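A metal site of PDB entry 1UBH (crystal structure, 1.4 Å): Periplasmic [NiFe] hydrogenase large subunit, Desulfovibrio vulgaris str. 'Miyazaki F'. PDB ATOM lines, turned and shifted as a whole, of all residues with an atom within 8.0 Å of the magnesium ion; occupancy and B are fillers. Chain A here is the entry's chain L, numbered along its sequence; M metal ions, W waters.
The side-chain amide oxygen of Gln 479 lies close to the side-chain carboxylate of Glu 44.
OG1 of Thr 339 lies within hydrogen-bond range of OE1 of Glu 44 (2.8 Å).
The backbone carbonyl oxygen (O) of Cys 531 sits at hydrogen-bond distance from a ring nitrogen (ND1) of His 534 (2.8 Å).
The nearest printed residue that does not touch the magnesium ion is Gln 479 (4.1 Å).
The magnesium ion is bound by water W2, water W1, water W3, O of Leu 480, OE2 of Glu 44 and NE2 of His 534.
The magnesium ion has six donor atoms within binding distance.
Water W1 bridges OE1 of Glu 44 and NZ of Lys 356.
Water W2 lies within hydrogen-bond range of the side-chain carboxylate of Glu 319 (2.6 Å), the side-chain amide oxygen of Gln 479 (2.7 Å) and the side-chain amino group of Lys 356 (3.0 Å).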
ATOM      1  N   PHE A  40      12.859 -33.967 -38.252  1.00  0.00           N
ATOM      2  CA  PHE A  40      13.037 -32.666 -37.626  1.00  0.00           C
ATOM      3  C   PHE A  40      11.702 -31.929 -37.602  1.00  0.00           C
ATOM      4  O   PHE A  40      10.987 -31.950 -38.621  1.00  0.00           O
ATOM      5  CB  PHE A  40      14.060 -31.870 -38.392  1.00  0.00           C
ATOM      6  CG  PHE A  40      14.291 -30.433 -37.917  1.00  0.00           C
ATOM      7  CD1 PHE A  40      15.083 -30.188 -36.825  1.00  0.00           C
ATOM      8  CD2 PHE A  40      13.693 -29.364 -38.573  1.00  0.00           C
ATOM      9  CE1 PHE A  40      15.331 -28.907 -36.367  1.00  0.00           C
ATOM     10  CE2 PHE A  40      13.943 -28.076 -38.123  1.00  0.00           C
ATOM     11  CZ  PHE A  40      14.733 -27.838 -37.024  1.00  0.00           C
ATOM     12  N   GLU A  44      12.211 -25.208 -31.417  1.00  0.00           N
ATOM     13  CA  GLU A  44      12.992 -24.064 -30.943  1.00  0.00           C
ATOM     14  C   GLU A  44      12.849 -22.853 -31.881  1.00  0.00           C
ATOM     15  O   GLU A  44      12.813 -21.705 -31.401  1.00  0.00           O
ATOM     16  CB  GLU A  44      14.454 -24.441 -30.783  1.00  0.00           C
ATOM     17  CG  GLU A  44      14.733 -25.481 -29.699  1.00  0.00           C
ATOM     18  CD  GLU A  44      15.954 -26.335 -29.883  1.00  0.00           C
ATOM     19  OE1 GLU A  44      16.369 -26.445 -31.057  1.00  0.00           O
ATOM     20  OE2 GLU A  44      16.421 -26.891 -28.888  1.00  0.00           O
ATOM     21  N   GLU A 319      26.504 -28.179 -27.374  1.00  0.00           N
ATOM     22  CA  GLU A 319      25.863 -29.041 -28.371  1.00  0.00           C
ATOM     23  C   GLU A 319      26.567 -28.870 -29.719  1.00  0.00           C
ATOM     24  O   GLU A 319      26.590 -27.759 -30.256  1.00  0.00           O
ATOM     25  CB  GLU A 319      24.374 -28.743 -28.458  1.00  0.00           C
ATOM     26  CG  GLU A 319      23.592 -29.146 -27.232  1.00  0.00           C
ATOM     27  CD  GLU A 319      22.103 -28.954 -27.487  1.00  0.00           C
ATOM     28  OE1 GLU A 319      21.431 -29.992 -27.644  1.00  0.00           O
ATOM     29  OE2 GLU A 319      21.627 -27.796 -27.564  1.00  0.00           O
ATOM     30  N   TYR A 326      22.844 -29.313 -39.459  1.00  0.00           N
ATOM     31  CA  TYR A 326      22.742 -27.908 -39.100  1.00  0.00           C
ATOM     32  C   TYR A 326      23.924 -27.172 -39.736  1.00  0.00           C
ATOM     33  O   TYR A 326      24.905 -27.777 -40.142  1.00  0.00           O
ATOM     34  CB  TYR A 326      22.692 -27.695 -37.586  1.00  0.00           C
ATOM     35  CG  TYR A 326      21.472 -28.373 -36.987  1.00  0.00           C
ATOM     36  CD1 TYR A 326      21.613 -29.620 -36.402  1.00  0.00           C
ATOM     37  CD2 TYR A 326      20.201 -27.818 -37.036  1.00  0.00           C
ATOM     38  CE1 TYR A 326      20.536 -30.258 -35.874  1.00  0.00           C
ATOM     39  CE2 TYR A 326      19.102 -28.465 -36.522  1.00  0.00           C
ATOM     40  CZ  TYR A 326      19.267 -29.696 -35.930  1.00  0.00           C
ATOM     41  OH  TYR A 326      18.193 -30.363 -35.401  1.00  0.00           O
ATOM     42  N   PRO A 334      23.770 -23.993 -24.597  1.00  0.00           N
ATOM     43  CA  PRO A 334      22.382 -23.715 -24.930  1.00  0.00           C
ATOM     44  C   PRO A 334      21.853 -22.308 -24.717  1.00  0.00           C
ATOM     45  O   PRO A 334      20.904 -21.872 -25.361  1.00  0.00           O
ATOM     46  CB  PRO A 334      21.582 -24.702 -24.057  1.00  0.00           C
ATOM     47  CG  PRO A 334      22.520 -25.569 -23.388  1.00  0.00           C
ATOM     48  CD  PRO A 334      23.902 -25.166 -23.723  1.00  0.00           C
ATOM     49  N   GLY A 337      22.545 -21.049 -27.918  1.00  0.00           N
ATOM     50  CA  GLY A 337      22.218 -22.072 -28.886  1.00  0.00           C
ATOM     51  C   GLY A 337      21.764 -21.527 -30.220  1.00  0.00           C
ATOM     52  O   GLY A 337      21.273 -20.396 -30.339  1.00  0.00           O
ATOM     53  N   GLN A 338      21.891 -22.389 -31.229  1.00  0.00           N
ATOM     54  CA  GLN A 338      21.510 -22.121 -32.584  1.00  0.00           C
ATOM     55  C   GLN A 338      20.797 -23.341 -33.183  1.00  0.00           C
ATOM     56  O   GLN A 338      21.280 -24.454 -32.980  1.00  0.00           O
ATOM     57  CB  GLN A 338      22.746 -21.823 -33.491  1.00  0.00           C
ATOM     58  CG  GLN A 338      23.488 -20.575 -33.013  1.00  0.00           C
ATOM     59  CD  GLN A 338      24.657 -20.249 -33.936  1.00  0.00           C
ATOM     60  OE1 GLN A 338      24.706 -19.166 -34.508  1.00  0.00           O
ATOM     61  NE2 GLN A 338      25.557 -21.213 -34.071  1.00  0.00           N
ATOM     62  N   THR A 339      19.706 -23.093 -33.895  1.00  0.00           N
ATOM     63  CA  THR A 339      19.010 -24.190 -34.610  1.00  0.00           C
ATOM     64  C   THR A 339      18.739 -23.752 -36.031  1.00  0.00           C
ATOM     65  O   THR A 339      17.716 -23.154 -36.320  1.00  0.00           O
ATOM     66  CB  THR A 339      17.761 -24.560 -33.800  1.00  0.00           C
ATOM     67  OG1 THR A 339      18.135 -24.760 -32.412  1.00  0.00           O
ATOM     68  CG2 THR A 339      17.158 -25.831 -34.340  1.00  0.00           C
ATOM     69  N   TRP A 354      19.518 -35.523 -37.440  1.00  0.00           N
ATOM     70  CA  TRP A 354      18.853 -34.263 -37.048  1.00  0.00           C
ATOM     71  C   TRP A 354      19.079 -33.910 -35.619  1.00  0.00           C
ATOM     72  O   TRP A 354      18.783 -32.870 -35.047  1.00  0.00           O
ATOM     73  CB  TRP A 354      17.354 -34.308 -37.332  1.00  0.00           C
ATOM     74  CG  TRP A 354      17.029 -34.120 -38.776  1.00  0.00           C
ATOM     75  CD1 TRP A 354      16.499 -35.032 -39.657  1.00  0.00           C
ATOM     76  CD2 TRP A 354      17.216 -32.934 -39.583  1.00  0.00           C
ATOM     77  NE1 TRP A 354      16.336 -34.504 -40.903  1.00  0.00           N
ATOM     78  CE2 TRP A 354      16.777 -33.217 -40.882  1.00  0.00           C
ATOM     79  CE3 TRP A 354      17.708 -31.673 -39.284  1.00  0.00           C
ATOM     80  CZ2 TRP A 354      16.840 -32.241 -41.896  1.00  0.00           C
ATOM     81  CZ3 TRP A 354      17.765 -30.725 -40.298  1.00  0.00           C
ATOM     82  CH2 TRP A 354      17.328 -31.001 -41.591  1.00  0.00           C
ATOM     83  N   MET A 355      19.577 -34.764 -34.757  1.00  0.00           N
ATOM     84  CA  MET A 355      20.030 -34.556 -33.427  1.00  0.00           C
ATOM     85  C   MET A 355      21.382 -33.835 -33.431  1.00  0.00           C
ATOM     86  O   MET A 355      22.295 -34.166 -34.177  1.00  0.00           O
ATOM     87  CB  MET A 355      20.154 -35.815 -32.594  1.00  0.00           C
ATOM     88  CG  MET A 355      18.890 -36.525 -32.215  1.00  0.00           C
ATOM     89  SD  MET A 355      19.205 -37.617 -30.811  1.00  0.00           S
ATOM     90  CE  MET A 355      17.788 -38.738 -30.890  1.00  0.00           C
ATOM     91  N   LYS A 356      21.448 -32.845 -32.536  1.00  0.00           N
ATOM     92  CA  LYS A 356      22.695 -32.250 -32.114  1.00  0.00           C
ATOM     93  C   LYS A 356      23.445 -33.260 -31.231  1.00  0.00           C
ATOM     94  O   LYS A 356      22.842 -34.270 -30.808  1.00  0.00           O
ATOM     95  CB  LYS A 356      22.505 -30.939 -31.336  1.00  0.00           C
ATOM     96  CG  LYS A 356      21.795 -29.879 -32.163  1.00  0.00           C
ATOM     97  CD  LYS A 356      21.544 -28.612 -31.371  1.00  0.00           C
ATOM     98  CE  LYS A 356      20.872 -27.516 -32.142  1.00  0.00           C
ATOM     99  NZ  LYS A 356      20.386 -26.427 -31.248  1.00  0.00           N
ATOM    100  N   PRO A 358      25.309 -33.373 -27.834  1.00  0.00           N
ATOM    101  CA  PRO A 358      25.685 -32.723 -26.552  1.00  0.00           C
ATOM    102  C   PRO A 358      26.931 -33.398 -25.970  1.00  0.00           C
ATOM    103  O   PRO A 358      27.055 -34.626 -25.965  1.00  0.00           O
ATOM    104  CB  PRO A 358      24.472 -32.917 -25.655  1.00  0.00           C
ATOM    105  CG  PRO A 358      23.358 -33.314 -26.583  1.00  0.00           C
ATOM    106  CD  PRO A 358      24.046 -34.095 -27.673  1.00  0.00           C
ATOM    107  N   SER A 465      16.986 -30.480 -19.948  1.00  0.00           N
ATOM    108  CA  SER A 465      17.106 -29.087 -19.593  1.00  0.00           C
ATOM    109  C   SER A 465      16.528 -28.199 -20.704  1.00  0.00           C
ATOM    110  O   SER A 465      16.729 -28.494 -21.862  1.00  0.00           O
ATOM    111  CB  SER A 465      18.540 -28.681 -19.319  1.00  0.00           C
ATOM    112  OG  SER A 465      19.459 -29.048 -20.319  1.00  0.00           O
ATOM    113  N   TRP A 467      16.233 -24.041 -21.698  1.00  0.00           N
ATOM    114  CA  TRP A 467      17.060 -22.848 -21.501  1.00  0.00           C
ATOM    115  C   TRP A 467      16.425 -21.671 -22.203  1.00  0.00           C
ATOM    116  O   TRP A 467      16.237 -21.781 -23.411  1.00  0.00           O
ATOM    117  CB  TRP A 467      18.451 -23.132 -22.044  1.00  0.00           C
ATOM    118  CG  TRP A 467      19.144 -24.341 -21.553  1.00  0.00           C
ATOM    119  CD1 TRP A 467      18.930 -25.641 -21.869  1.00  0.00           C
ATOM    120  CD2 TRP A 467      20.234 -24.337 -20.608  1.00  0.00           C
ATOM    121  NE1 TRP A 467      19.803 -26.428 -21.181  1.00  0.00           N
ATOM    122  CE2 TRP A 467      20.609 -25.666 -20.407  1.00  0.00           C
ATOM    123  CE3 TRP A 467      20.910 -23.331 -19.926  1.00  0.00           C
ATOM    124  CZ2 TRP A 467      21.650 -25.993 -19.532  1.00  0.00           C
ATOM    125  CZ3 TRP A 467      21.925 -23.639 -19.080  1.00  0.00           C
ATOM    126  CH2 TRP A 467      22.278 -24.978 -18.893  1.00  0.00           C
ATOM    127  N   PHE A 478      15.187 -20.049 -27.103  1.00  0.00           N
ATOM    128  CA  PHE A 478      14.711 -21.149 -26.281  1.00  0.00           C
ATOM    129  C   PHE A 478      15.363 -22.439 -26.814  1.00  0.00           C
ATOM    130  O   PHE A 478      15.165 -22.734 -27.975  1.00  0.00           O
ATOM    131  CB  PHE A 478      13.186 -21.247 -26.287  1.00  0.00           C
ATOM    132  CG  PHE A 478      12.653 -22.016 -25.099  1.00  0.00           C
ATOM    133  CD1 PHE A 478      12.817 -23.379 -24.949  1.00  0.00           C
ATOM    134  CD2 PHE A 478      11.970 -21.360 -24.098  1.00  0.00           C
ATOM    135  CE1 PHE A 478      12.334 -24.067 -23.855  1.00  0.00           C
ATOM    136  CE2 PHE A 478      11.473 -22.016 -22.990  1.00  0.00           C
ATOM    137  CZ  PHE A 478      11.688 -23.383 -22.846  1.00  0.00           C
ATOM    138  N   GLN A 479      16.096 -23.106 -25.989  1.00  0.00           N
ATOM    139  CA  GLN A 479      16.830 -24.330 -26.389  1.00  0.00           C
ATOM    140  C   GLN A 479      16.484 -25.486 -25.450  1.00  0.00           C
ATOM    141  O   GLN A 479      16.509 -25.325 -24.230  1.00  0.00           O
ATOM    142  CB  GLN A 479      18.345 -24.043 -26.387  1.00  0.00           C
ATOM    143  CG  GLN A 479      18.764 -23.036 -27.448  1.00  0.00           C
ATOM    144  CD  GLN A 479      18.662 -23.517 -28.858  1.00  0.00           C
ATOM    145  OE1 GLN A 479      18.905 -24.690 -29.123  1.00  0.00           O
ATOM    146  NE2 GLN A 479      18.340 -22.615 -29.776  1.00  0.00           N
ATOM    147  N   LEU A 480      16.151 -26.608 -26.097  1.00  0.00           N
ATOM    148  CA  LEU A 480      15.951 -27.858 -25.367  1.00  0.00           C
ATOM    149  C   LEU A 480      17.169 -28.726 -25.579  1.00  0.00           C
ATOM    150  O   LEU A 480      17.632 -28.844 -26.667  1.00  0.00           O
ATOM    151  CB  LEU A 480      14.727 -28.590 -25.885  1.00  0.00           C
ATOM    152  CG  LEU A 480      13.351 -27.985 -25.731  1.00  0.00           C
ATOM    153  CD1 LEU A 480      13.154 -26.836 -26.682  1.00  0.00           C
ATOM    154  CD2 LEU A 480      12.239 -29.039 -26.013  1.00  0.00           C
ATOM    155  N   VAL A 481      17.644 -29.340 -24.525  1.00  0.00           N
ATOM    156  CA  VAL A 481      18.714 -30.310 -24.560  1.00  0.00           C
ATOM    157  C   VAL A 481      18.133 -31.527 -23.827  1.00  0.00           C
ATOM    158  O   VAL A 481      17.878 -31.480 -22.622  1.00  0.00           O
ATOM    159  CB  VAL A 481      20.008 -29.857 -23.885  1.00  0.00           C
ATOM    160  CG1 VAL A 481      21.098 -30.936 -24.044  1.00  0.00           C
ATOM    161  CG2 VAL A 481      20.428 -28.521 -24.446  1.00  0.00           C
ATOM    162  N   VAL A 482      17.895 -32.594 -24.595  1.00  0.00           N
ATOM    163  CA  VAL A 482      17.000 -33.618 -24.069  1.00  0.00           C
ATOM    164  C   VAL A 482      17.742 -34.902 -23.816  1.00  0.00           C
ATOM    165  O   VAL A 482      18.781 -35.111 -24.422  1.00  0.00           O
ATOM    166  CB  VAL A 482      15.877 -33.733 -25.125  1.00  0.00           C
ATOM    167  CG1 VAL A 482      14.777 -34.681 -24.737  1.00  0.00           C
ATOM    168  CG2 VAL A 482      15.221 -32.382 -25.379  1.00  0.00           C
ATOM    169  N   THR A 485      18.939 -36.784 -26.719  1.00  0.00           N
ATOM    170  CA  THR A 485      19.931 -36.039 -27.498  1.00  0.00           C
ATOM    171  C   THR A 485      21.309 -36.441 -27.006  1.00  0.00           C
ATOM    172  O   THR A 485      22.233 -36.723 -27.746  1.00  0.00           O
ATOM    173  CB  THR A 485      19.777 -34.512 -27.355  1.00  0.00           C
ATOM    174  OG1 THR A 485      18.399 -34.163 -27.329  1.00  0.00           O
ATOM    175  CG2 THR A 485      20.502 -33.797 -28.469  1.00  0.00           C
ATOM    176  N   CYS A 531      11.820 -36.409 -28.799  1.00  0.00           N
ATOM    177  CA  CYS A 531      12.560 -35.748 -27.747  1.00  0.00           C
ATOM    178  C   CYS A 531      13.930 -35.309 -28.204  1.00  0.00           C
ATOM    179  O   CYS A 531      14.364 -34.183 -28.002  1.00  0.00           O
ATOM    180  CB  CYS A 531      12.760 -36.770 -26.580  1.00  0.00           C
ATOM    181  SG  CYS A 531      11.454 -36.568 -25.376  1.00  0.00           S
ATOM    182  N   GLY A 532      14.683 -36.232 -28.844  1.00  0.00           N
ATOM    183  CA  GLY A 532      16.075 -35.916 -29.078  1.00  0.00           C
ATOM    184  C   GLY A 532      16.239 -34.803 -30.081  1.00  0.00           C
ATOM    185  O   GLY A 532      17.210 -34.039 -29.934  1.00  0.00           O
ATOM    186  N   VAL A 533      15.358 -34.693 -31.055  1.00  0.00           N
ATOM    187  CA  VAL A 533      15.485 -33.710 -32.119  1.00  0.00           C
ATOM    188  C   VAL A 533      14.657 -32.457 -31.947  1.00  0.00           C
ATOM    189  O   VAL A 533      15.100 -31.320 -32.163  1.00  0.00           O
ATOM    190  CB  VAL A 533      15.068 -34.275 -33.509  1.00  0.00           C
ATOM    191  CG1 VAL A 533      15.164 -33.252 -34.652  1.00  0.00           C
ATOM    192  CG2 VAL A 533      15.933 -35.511 -33.836  1.00  0.00           C
ATOM    193  N   HIS A 534      13.392 -32.600 -31.512  1.00  0.00           N
ATOM    194  CA  HIS A 534      12.434 -31.519 -31.267  1.00  0.00           C
ATOM    195  C   HIS A 534      12.437 -30.549 -32.466  1.00  0.00           C
ATOM    196  O   HIS A 534      12.431 -31.191 -33.659  1.00  0.00           O
ATOM    197  CB  HIS A 534      12.583 -30.775 -29.947  1.00  0.00           C
ATOM    198  CG  HIS A 534      13.998 -30.535 -29.471  1.00  0.00           C
ATOM    199  ND1 HIS A 534      14.770 -31.564 -28.906  1.00  0.00           N
ATOM    200  CD2 HIS A 534      14.821 -29.477 -29.567  1.00  0.00           C
ATOM    201  CE1 HIS A 534      15.969 -31.107 -28.650  1.00  0.00           C
ATOM    202  NE2 HIS A 534      16.017 -29.868 -29.035  1.00  0.00           N
ATOM    203  OXT HIS A 534      12.409 -29.349 -32.447  1.00  0.00           O
HETATM  204 MG    MG M   1      17.761 -28.596 -28.802  1.00  0.00          MG
HETATM  205  O   HOH W   1      18.152 -28.359 -30.819  1.00  0.00           O
HETATM  206  O   HOH W   2      19.329 -27.288 -28.613  1.00  0.00           O
HETATM  207  O   HOH W   3      19.079 -30.263 -28.794  1.00  0.00           O
